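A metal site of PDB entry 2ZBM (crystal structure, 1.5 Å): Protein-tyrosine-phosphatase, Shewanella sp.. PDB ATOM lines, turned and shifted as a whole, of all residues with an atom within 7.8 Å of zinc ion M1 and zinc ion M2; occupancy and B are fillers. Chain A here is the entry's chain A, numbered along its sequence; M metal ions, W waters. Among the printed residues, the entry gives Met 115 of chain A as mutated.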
ATOM      1  N   SER A  77     -21.590   8.032  13.787  1.00  0.00           N
ATOM      2  CA  SER A  77     -21.852   9.175  12.896  1.00  0.00           C
ATOM      3  C   SER A  77     -20.629  10.024  12.625  1.00  0.00           C
ATOM      4  O   SER A  77     -19.691   9.901  13.430  1.00  0.00           O
ATOM      5  CB  SER A  77     -22.896  10.107  13.546  1.00  0.00           C
ATOM      6  OG  SER A  77     -23.514  10.950  12.583  1.00  0.00           O
ATOM      7  N   ASP A  78     -20.672  10.855  11.590  1.00  0.00           N
ATOM      8  CA  ASP A  78     -19.679  11.938  11.463  1.00  0.00           C
ATOM      9  C   ASP A  78     -18.250  11.388  11.461  1.00  0.00           C
ATOM     10  O   ASP A  78     -17.339  11.907  12.099  1.00  0.00           O
ATOM     11  CB  ASP A  78     -19.866  13.040  12.538  1.00  0.00           C
ATOM     12  CG  ASP A  78     -21.205  13.732  12.381  1.00  0.00           C
ATOM     13  OD1 ASP A  78     -21.295  14.790  11.730  1.00  0.00           O
ATOM     14  OD2 ASP A  78     -22.213  13.170  12.950  1.00  0.00           O
ATOM     15  N   VAL A  79     -18.058  10.336  10.648  1.00  0.00           N
ATOM     16  CA  VAL A  79     -16.692   9.798  10.470  1.00  0.00           C
ATOM     17  C   VAL A  79     -15.793  10.810   9.780  1.00  0.00           C
ATOM     18  O   VAL A  79     -14.572  10.878  10.063  1.00  0.00           O
ATOM     19  CB  VAL A  79     -16.791   8.478   9.672  1.00  0.00           C
ATOM     20  CG1 VAL A  79     -15.424   7.996   9.215  1.00  0.00           C
ATOM     21  CG2 VAL A  79     -17.498   7.400  10.512  1.00  0.00           C
ATOM     22  N   HIS A  80     -16.331  11.657   8.894  1.00  0.00           N
ATOM     23  CA  HIS A  80     -15.561  12.748   8.269  1.00  0.00           C
ATOM     24  C   HIS A  80     -14.218  12.291   7.726  1.00  0.00           C
ATOM     25  O   HIS A  80     -13.151  12.845   8.085  1.00  0.00           O
ATOM     26  CB  HIS A  80     -15.444  13.948   9.276  1.00  0.00           C
ATOM     27  CG  HIS A  80     -16.718  14.740   9.345  1.00  0.00           C
ATOM     28  ND1 HIS A  80     -17.300  15.323   8.221  1.00  0.00           N
ATOM     29  CD2 HIS A  80     -17.553  15.053  10.394  1.00  0.00           C
ATOM     30  CE1 HIS A  80     -18.400  15.942   8.605  1.00  0.00           C
ATOM     31  NE2 HIS A  80     -18.595  15.801   9.908  1.00  0.00           N
ATOM     32  N   THR A 112     -25.354   7.756  10.890  1.00  0.00           N
ATOM     33  CA  THR A 112     -26.251   8.884  10.706  1.00  0.00           C
ATOM     34  C   THR A 112     -25.576  10.050  10.001  1.00  0.00           C
ATOM     35  O   THR A 112     -25.728  11.188  10.490  1.00  0.00           O
ATOM     36  CB  THR A 112     -26.874   9.354  12.040  1.00  0.00           C
ATOM     37  OG1 THR A 112     -25.840   9.661  12.979  1.00  0.00           O
ATOM     38  CG2 THR A 112     -27.697   8.224  12.674  1.00  0.00           C
ATOM     39  N   GLY A 113     -24.852   9.819   8.888  1.00  0.00           N
ATOM     40  CA  GLY A 113     -24.400  10.871   8.024  1.00  0.00           C
ATOM     41  C   GLY A 113     -22.952  11.316   8.224  1.00  0.00           C
ATOM     42  O   GLY A 113     -22.263  10.911   9.175  1.00  0.00           O
ATOM     43  N   ASP A 114     -22.507  12.190   7.306  1.00  0.00           N
ATOM     44  CA  ASP A 114     -21.228  12.867   7.341  1.00  0.00           C
ATOM     45  C   ASP A 114     -20.026  11.926   7.292  1.00  0.00           C
ATOM     46  O   ASP A 114     -19.069  11.992   8.110  1.00  0.00           O
ATOM     47  CB  ASP A 114     -21.136  13.786   8.581  1.00  0.00           C
ATOM     48  CG  ASP A 114     -21.764  15.146   8.312  1.00  0.00           C
ATOM     49  OD1 ASP A 114     -21.619  16.042   9.161  1.00  0.00           O
ATOM     50  OD2 ASP A 114     -22.490  15.298   7.294  1.00  0.00           O
ATOM     51  N   MET A 115     -20.050  11.115   6.242  1.00  0.00           N
ATOM     52  CA  MET A 115     -18.895  10.335   5.875  1.00  0.00           C
ATOM     53  C   MET A 115     -17.856  11.234   5.168  1.00  0.00           C
ATOM     54  O   MET A 115     -16.633  11.047   5.346  1.00  0.00           O
ATOM     55  CB  MET A 115     -19.196   9.164   4.933  1.00  0.00           C
ATOM     56  CG  MET A 115     -20.002   8.047   5.634  1.00  0.00           C
ATOM     57  SD  MET A 115     -20.583   6.826   4.430  1.00  0.00           S
ATOM     58  CE  MET A 115     -21.795   7.801   3.526  1.00  0.00           C
ATOM     59  N   PHE A 116     -18.350  12.202   4.378  1.00  0.00           N
ATOM     60  CA  PHE A 116     -17.479  13.082   3.643  1.00  0.00           C
ATOM     61  C   PHE A 116     -16.855  14.194   4.482  1.00  0.00           C
ATOM     62  O   PHE A 116     -17.394  14.526   5.541  1.00  0.00           O
ATOM     63  CB  PHE A 116     -18.301  13.813   2.589  1.00  0.00           C
ATOM     64  CG  PHE A 116     -18.616  12.959   1.378  1.00  0.00           C
ATOM     65  CD1 PHE A 116     -19.795  12.198   1.335  1.00  0.00           C
ATOM     66  CD2 PHE A 116     -17.741  12.944   0.307  1.00  0.00           C
ATOM     67  CE1 PHE A 116     -20.063  11.444   0.213  1.00  0.00           C
ATOM     68  CE2 PHE A 116     -18.020  12.206  -0.826  1.00  0.00           C
ATOM     69  CZ  PHE A 116     -19.205  11.482  -0.908  1.00  0.00           C
ATOM     70  N   ASP A 117     -15.815  14.819   3.995  1.00  0.00           N
ATOM     71  CA  ASP A 117     -15.274  16.106   4.350  1.00  0.00           C
ATOM     72  C   ASP A 117     -14.399  16.043   5.618  1.00  0.00           C
ATOM     73  O   ASP A 117     -14.499  15.141   6.450  1.00  0.00           O
ATOM     74  CB  ASP A 117     -16.377  17.163   4.464  1.00  0.00           C
ATOM     75  CG  ASP A 117     -16.883  17.639   3.093  1.00  0.00           C
ATOM     76  OD1 ASP A 117     -17.821  18.471   3.053  1.00  0.00           O
ATOM     77  OD2 ASP A 117     -16.342  17.204   2.048  1.00  0.00           O
ATOM     78  N   GLY A 148     -26.074  12.977   5.572  1.00  0.00           N
ATOM     79  CA  GLY A 148     -25.828  14.089   6.528  1.00  0.00           C
ATOM     80  C   GLY A 148     -25.702  15.387   5.733  1.00  0.00           C
ATOM     81  O   GLY A 148     -25.805  15.440   4.471  1.00  0.00           O
ATOM     82  N   ASN A 149     -25.430  16.498   6.403  1.00  0.00           N
ATOM     83  CA  ASN A 149     -25.325  17.776   5.697  1.00  0.00           C
ATOM     84  C   ASN A 149     -24.093  17.751   4.774  1.00  0.00           C
ATOM     85  O   ASN A 149     -24.180  18.361   3.701  1.00  0.00           O
ATOM     86  CB  ASN A 149     -25.342  18.988   6.644  1.00  0.00           C
ATOM     87  CG  ASN A 149     -24.163  19.099   7.573  1.00  0.00           C
ATOM     88  OD1 ASN A 149     -23.525  20.162   7.702  1.00  0.00           O
ATOM     89  ND2 ASN A 149     -23.877  18.006   8.255  1.00  0.00           N
ATOM     90  N   HIS A 150     -23.025  17.051   5.128  1.00  0.00           N
ATOM     91  CA  HIS A 150     -21.869  17.072   4.191  1.00  0.00           C
ATOM     92  C   HIS A 150     -22.119  16.196   2.959  1.00  0.00           C
ATOM     93  O   HIS A 150     -21.621  16.546   1.850  1.00  0.00           O
ATOM     94  CB  HIS A 150     -20.637  16.630   4.936  1.00  0.00           C
ATOM     95  CG  HIS A 150     -20.175  17.795   5.803  1.00  0.00           C
ATOM     96  ND1 HIS A 150     -19.160  18.644   5.405  1.00  0.00           N
ATOM     97  CD2 HIS A 150     -20.625  18.224   6.991  1.00  0.00           C
ATOM     98  CE1 HIS A 150     -19.001  19.579   6.383  1.00  0.00           C
ATOM     99  NE2 HIS A 150     -19.869  19.342   7.357  1.00  0.00           N
ATOM    100  N   GLU A 151     -22.874  15.109   3.081  1.00  0.00           N
ATOM    101  CA  GLU A 151     -23.284  14.410   1.837  1.00  0.00           C
ATOM    102  C   GLU A 151     -24.044  15.357   0.904  1.00  0.00           C
ATOM    103  O   GLU A 151     -23.829  15.364  -0.318  1.00  0.00           O
ATOM    104  CB  GLU A 151     -24.122  13.158   2.065  1.00  0.00           C
ATOM    105  CG  GLU A 151     -23.327  11.937   2.510  1.00  0.00           C
ATOM    106  CD  GLU A 151     -22.776  12.118   3.924  1.00  0.00           C
ATOM    107  OE1 GLU A 151     -21.661  11.594   4.172  1.00  0.00           O
ATOM    108  OE2 GLU A 151     -23.471  12.745   4.763  1.00  0.00           O
ATOM    109  N   MET A 153     -23.994  18.645   0.879  1.00  0.00           N
ATOM    110  CA  MET A 153     -23.096  19.706   0.365  1.00  0.00           C
ATOM    111  C   MET A 153     -22.225  19.164  -0.752  1.00  0.00           C
ATOM    112  O   MET A 153     -22.150  19.786  -1.837  1.00  0.00           O
ATOM    113  CB  MET A 153     -22.243  20.321   1.477  1.00  0.00           C
ATOM    114  CG  MET A 153     -23.068  21.389   2.194  1.00  0.00           C
ATOM    115  SD  MET A 153     -22.123  22.300   3.396  1.00  0.00           S
ATOM    116  CE  MET A 153     -21.823  21.107   4.703  1.00  0.00           C
ATOM    117  N   HIS A 207     -29.454  12.919  10.939  1.00  0.00           N
ATOM    118  CA  HIS A 207     -28.152  13.508  11.162  1.00  0.00           C
ATOM    119  C   HIS A 207     -28.221  14.644  12.170  1.00  0.00           C
ATOM    120  O   HIS A 207     -27.413  14.631  13.133  1.00  0.00           O
ATOM    121  CB  HIS A 207     -27.638  14.017   9.798  1.00  0.00           C
ATOM    122  CG  HIS A 207     -26.245  14.611   9.973  1.00  0.00           C
ATOM    123  ND1 HIS A 207     -25.184  13.818  10.375  1.00  0.00           N
ATOM    124  CD2 HIS A 207     -25.786  15.863   9.862  1.00  0.00           C
ATOM    125  CE1 HIS A 207     -24.134  14.573  10.481  1.00  0.00           C
ATOM    126  NE2 HIS A 207     -24.426  15.842  10.167  1.00  0.00           N
ATOM    127  N   GLY A 208     -29.121  15.619  11.959  1.00  0.00           N
ATOM    128  CA  GLY A 208     -29.079  16.822  12.830  1.00  0.00           C
ATOM    129  C   GLY A 208     -30.108  16.787  13.929  1.00  0.00           C
ATOM    130  O   GLY A 208     -29.833  16.843  15.163  1.00  0.00           O
ATOM    131  N   THR A 255     -31.093  17.822   8.588  1.00  0.00           N
ATOM    132  CA  THR A 255     -29.653  17.522   8.498  1.00  0.00           C
ATOM    133  C   THR A 255     -28.825  18.672   9.038  1.00  0.00           C
ATOM    134  O   THR A 255     -27.610  18.452   9.128  1.00  0.00           O
ATOM    135  CB  THR A 255     -29.184  17.191   7.070  1.00  0.00           C
ATOM    136  OG1 THR A 255     -29.607  18.274   6.235  1.00  0.00           O
ATOM    137  CG2 THR A 255     -29.841  15.912   6.571  1.00  0.00           C
ATOM    138  N   TRP A 256     -29.388  19.823   9.389  1.00  0.00           N
ATOM    139  CA  TRP A 256     -28.563  20.881   9.963  1.00  0.00           C
ATOM    140  C   TRP A 256     -28.989  21.256  11.364  1.00  0.00           C
ATOM    141  O   TRP A 256     -28.199  21.923  12.080  1.00  0.00           O
ATOM    142  CB  TRP A 256     -28.601  22.168   9.103  1.00  0.00           C
ATOM    143  CG  TRP A 256     -27.812  22.112   7.823  1.00  0.00           C
ATOM    144  CD1 TRP A 256     -28.212  21.641   6.596  1.00  0.00           C
ATOM    145  CD2 TRP A 256     -26.461  22.569   7.651  1.00  0.00           C
ATOM    146  NE1 TRP A 256     -27.185  21.768   5.673  1.00  0.00           N
ATOM    147  CE2 TRP A 256     -26.106  22.335   6.310  1.00  0.00           C
ATOM    148  CE3 TRP A 256     -25.572  23.143   8.571  1.00  0.00           C
ATOM    149  CZ2 TRP A 256     -24.856  22.671   5.822  1.00  0.00           C
ATOM    150  CZ3 TRP A 256     -24.331  23.476   8.087  1.00  0.00           C
ATOM    151  CH2 TRP A 256     -23.975  23.242   6.745  1.00  0.00           C
ATOM    152  N   ARG A 258     -29.495  22.013  15.107  1.00  0.00           N
ATOM    153  CA  ARG A 258     -28.735  21.688  16.285  1.00  0.00           C
ATOM    154  C   ARG A 258     -29.508  22.002  17.541  1.00  0.00           C
ATOM    155  O   ARG A 258     -28.914  22.069  18.635  1.00  0.00           O
ATOM    156  CB  ARG A 258     -27.434  22.527  16.272  1.00  0.00           C
ATOM    157  CG  ARG A 258     -26.574  22.193  15.042  1.00  0.00           C
ATOM    158  CD  ARG A 258     -25.151  22.736  15.251  1.00  0.00           C
ATOM    159  NE  ARG A 258     -24.451  22.864  13.995  1.00  0.00           N
ATOM    160  CZ  ARG A 258     -23.567  21.937  13.616  1.00  0.00           C
ATOM    161  NH1 ARG A 258     -22.951  22.102  12.472  1.00  0.00           N
ATOM    162  NH2 ARG A 258     -23.376  20.910  14.430  1.00  0.00           N
ATOM    163  N   GLY A 285     -26.455  12.819  15.068  1.00  0.00           N
ATOM    164  CA  GLY A 285     -25.013  13.101  14.958  1.00  0.00           C
ATOM    165  C   GLY A 285     -24.794  14.592  14.873  1.00  0.00           C
ATOM    166  O   GLY A 285     -25.408  15.317  15.678  1.00  0.00           O
ATOM    167  N   HIS A 286     -23.989  15.069  13.964  1.00  0.00           N
ATOM    168  CA  HIS A 286     -23.859  16.443  13.468  1.00  0.00           C
ATOM    169  C   HIS A 286     -23.198  17.404  14.461  1.00  0.00           C
ATOM    170  O   HIS A 286     -22.292  18.159  14.040  1.00  0.00           O
ATOM    171  CB  HIS A 286     -25.233  16.991  13.074  1.00  0.00           C
ATOM    172  CG  HIS A 286     -25.207  18.343  12.416  1.00  0.00           C
ATOM    173  ND1 HIS A 286     -24.463  18.723  11.290  1.00  0.00           N
ATOM    174  CD2 HIS A 286     -25.911  19.447  12.779  1.00  0.00           C
ATOM    175  CE1 HIS A 286     -24.737  20.004  11.021  1.00  0.00           C
ATOM    176  NE2 HIS A 286     -25.618  20.466  11.919  1.00  0.00           N
ATOM    177  N   THR A 287     -23.641  17.438  15.709  1.00  0.00           N
ATOM    178  CA  THR A 287     -23.060  18.300  16.736  1.00  0.00           C
ATOM    179  C   THR A 287     -22.109  17.501  17.634  1.00  0.00           C
ATOM    180  O   THR A 287     -22.538  16.651  18.430  1.00  0.00           O
ATOM    181  CB  THR A 287     -24.197  18.932  17.562  1.00  0.00           C
ATOM    182  OG1 THR A 287     -25.132  19.522  16.642  1.00  0.00           O
ATOM    183  CG2 THR A 287     -23.699  20.031  18.487  1.00  0.00           C
ATOM    184  N   SER A 288     -20.793  17.774  17.444  1.00  0.00           N
ATOM    185  CA  SER A 288     -19.803  16.830  17.965  1.00  0.00           C
ATOM    186  C   SER A 288     -19.636  16.848  19.482  1.00  0.00           C
ATOM    187  O   SER A 288     -19.547  17.938  20.042  1.00  0.00           O
ATOM    188  CB  SER A 288     -18.437  17.172  17.363  1.00  0.00           C
ATOM    189  OG  SER A 288     -18.556  17.128  15.932  1.00  0.00           O
ATOM    190  N   ASP A 304     -22.422  11.694  17.416  1.00  0.00           N
ATOM    191  CA  ASP A 304     -21.217  12.327  16.874  1.00  0.00           C
ATOM    192  C   ASP A 304     -20.209  12.383  18.038  1.00  0.00           C
ATOM    193  O   ASP A 304     -20.366  13.243  18.927  1.00  0.00           O
ATOM    194  CB  ASP A 304     -21.461  13.692  16.208  1.00  0.00           C
ATOM    195  CG  ASP A 304     -20.174  14.321  15.667  1.00  0.00           C
ATOM    196  OD1 ASP A 304     -20.238  15.364  14.987  1.00  0.00           O
ATOM    197  OD2 ASP A 304     -19.055  13.775  15.908  1.00  0.00           O
ATOM    198  N   LYS A 308     -14.186  12.855  13.796  1.00  0.00           N
ATOM    199  CA  LYS A 308     -13.571  13.762  12.847  1.00  0.00           C
ATOM    200  C   LYS A 308     -12.184  14.244  13.283  1.00  0.00           C
ATOM    201  O   LYS A 308     -11.361  14.638  12.431  1.00  0.00           O
ATOM    202  CB  LYS A 308     -14.464  15.004  12.623  1.00  0.00           C
ATOM    203  CG  LYS A 308     -14.556  15.911  13.850  1.00  0.00           C
ATOM    204  CD  LYS A 308     -15.610  16.991  13.619  1.00  0.00           C
ATOM    205  CE  LYS A 308     -15.620  17.935  14.827  1.00  0.00           C
ATOM    206  NZ  LYS A 308     -16.669  18.974  14.802  1.00  0.00           N
HETATM  207 ZN    ZN M   1     -20.307  16.225  10.935  1.00  0.00          ZN
HETATM  208 ZN    ZN M   2     -23.186  17.443  10.114  1.00  0.00          ZN
HETATM  209  O   HOH W   1     -21.322  20.232   9.624  1.00  0.00           O
HETATM  210  O   HOH W   2     -19.310  16.608  12.697  1.00  0.00           O
HETATM  211  O   HOH W   3     -21.449  17.729  11.076  1.00  0.00           O
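The backbone NH of His 286 is in hydrogen-bond range of the side-chain carboxylate of Asp 78, at 2.8 Å.
The backbone carbonyl oxygen (O) of Gly 113 is in hydrogen-bond range of the backbone NH (N) of Asp 78 (2.9 Å).
N of Gly 285 sits at hydrogen-bond distance from O of His 207, at 2.8 Å.
The backbone carbonyl oxygen (O) of Thr 112 is in hydrogen-bond range of a ring nitrogen (ND1) of His 207 (2.7 Å).
O of Phe 116 sits at hydrogen-bond distance from ND1 of His 80.
The backbone carbonyl oxygen of His 286 is in hydrogen-bond range of the guanidinium group of Arg 258, 3.0 Å away.
NE2 of His 286 lies within hydrogen-bond range of O of Trp 256 (3.0 Å).
N of Val 79 sits at hydrogen-bond distance from O of Asp 114.
Of the 26 residues printed, 3 come within 4 Å of zinc ion M1.
Within 4 Å of zinc ion M2: Asp 78, Asp 114, Asn 149, His 207 and His 286.
Water W3 binds zinc ion M1 (1.9 Å).
OD1 of Asp 78 is bound to zinc ion M1 (1.9 Å).
Zinc ion M1 is bound by NE2 of His 80 (2.0 Å).
Water W2 binds zinc ion M1.
Zinc ion M1 is bound by OD1 of Asp 114, at 2.2 Å.
Zinc ion M1 has five donor atoms within binding distance.
Zinc ion M2 is bound by water W3 (2.0 Å).
Zinc ion M2 is bound by a ring nitrogen (NE2) of His 207, 2.0 Å away.
Zinc ion M2 is bound by ND2 of Asn 149, at 2.1 Å.
ND1 of His 286 binds zinc ion M2 (2.2 Å).
The side-chain carboxylate (OD1) of Asp 114 binds zinc ion M2 (2.3 Å).
Water W2 lies within hydrogen-bond range of OD1 of Asp 304 and OG of Ser 288.
Water W1 bridges a ring nitrogen (NE2) of His 150 (2.8 Å) and the side-chain amide oxygen of Asn 149 (2.9 Å).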
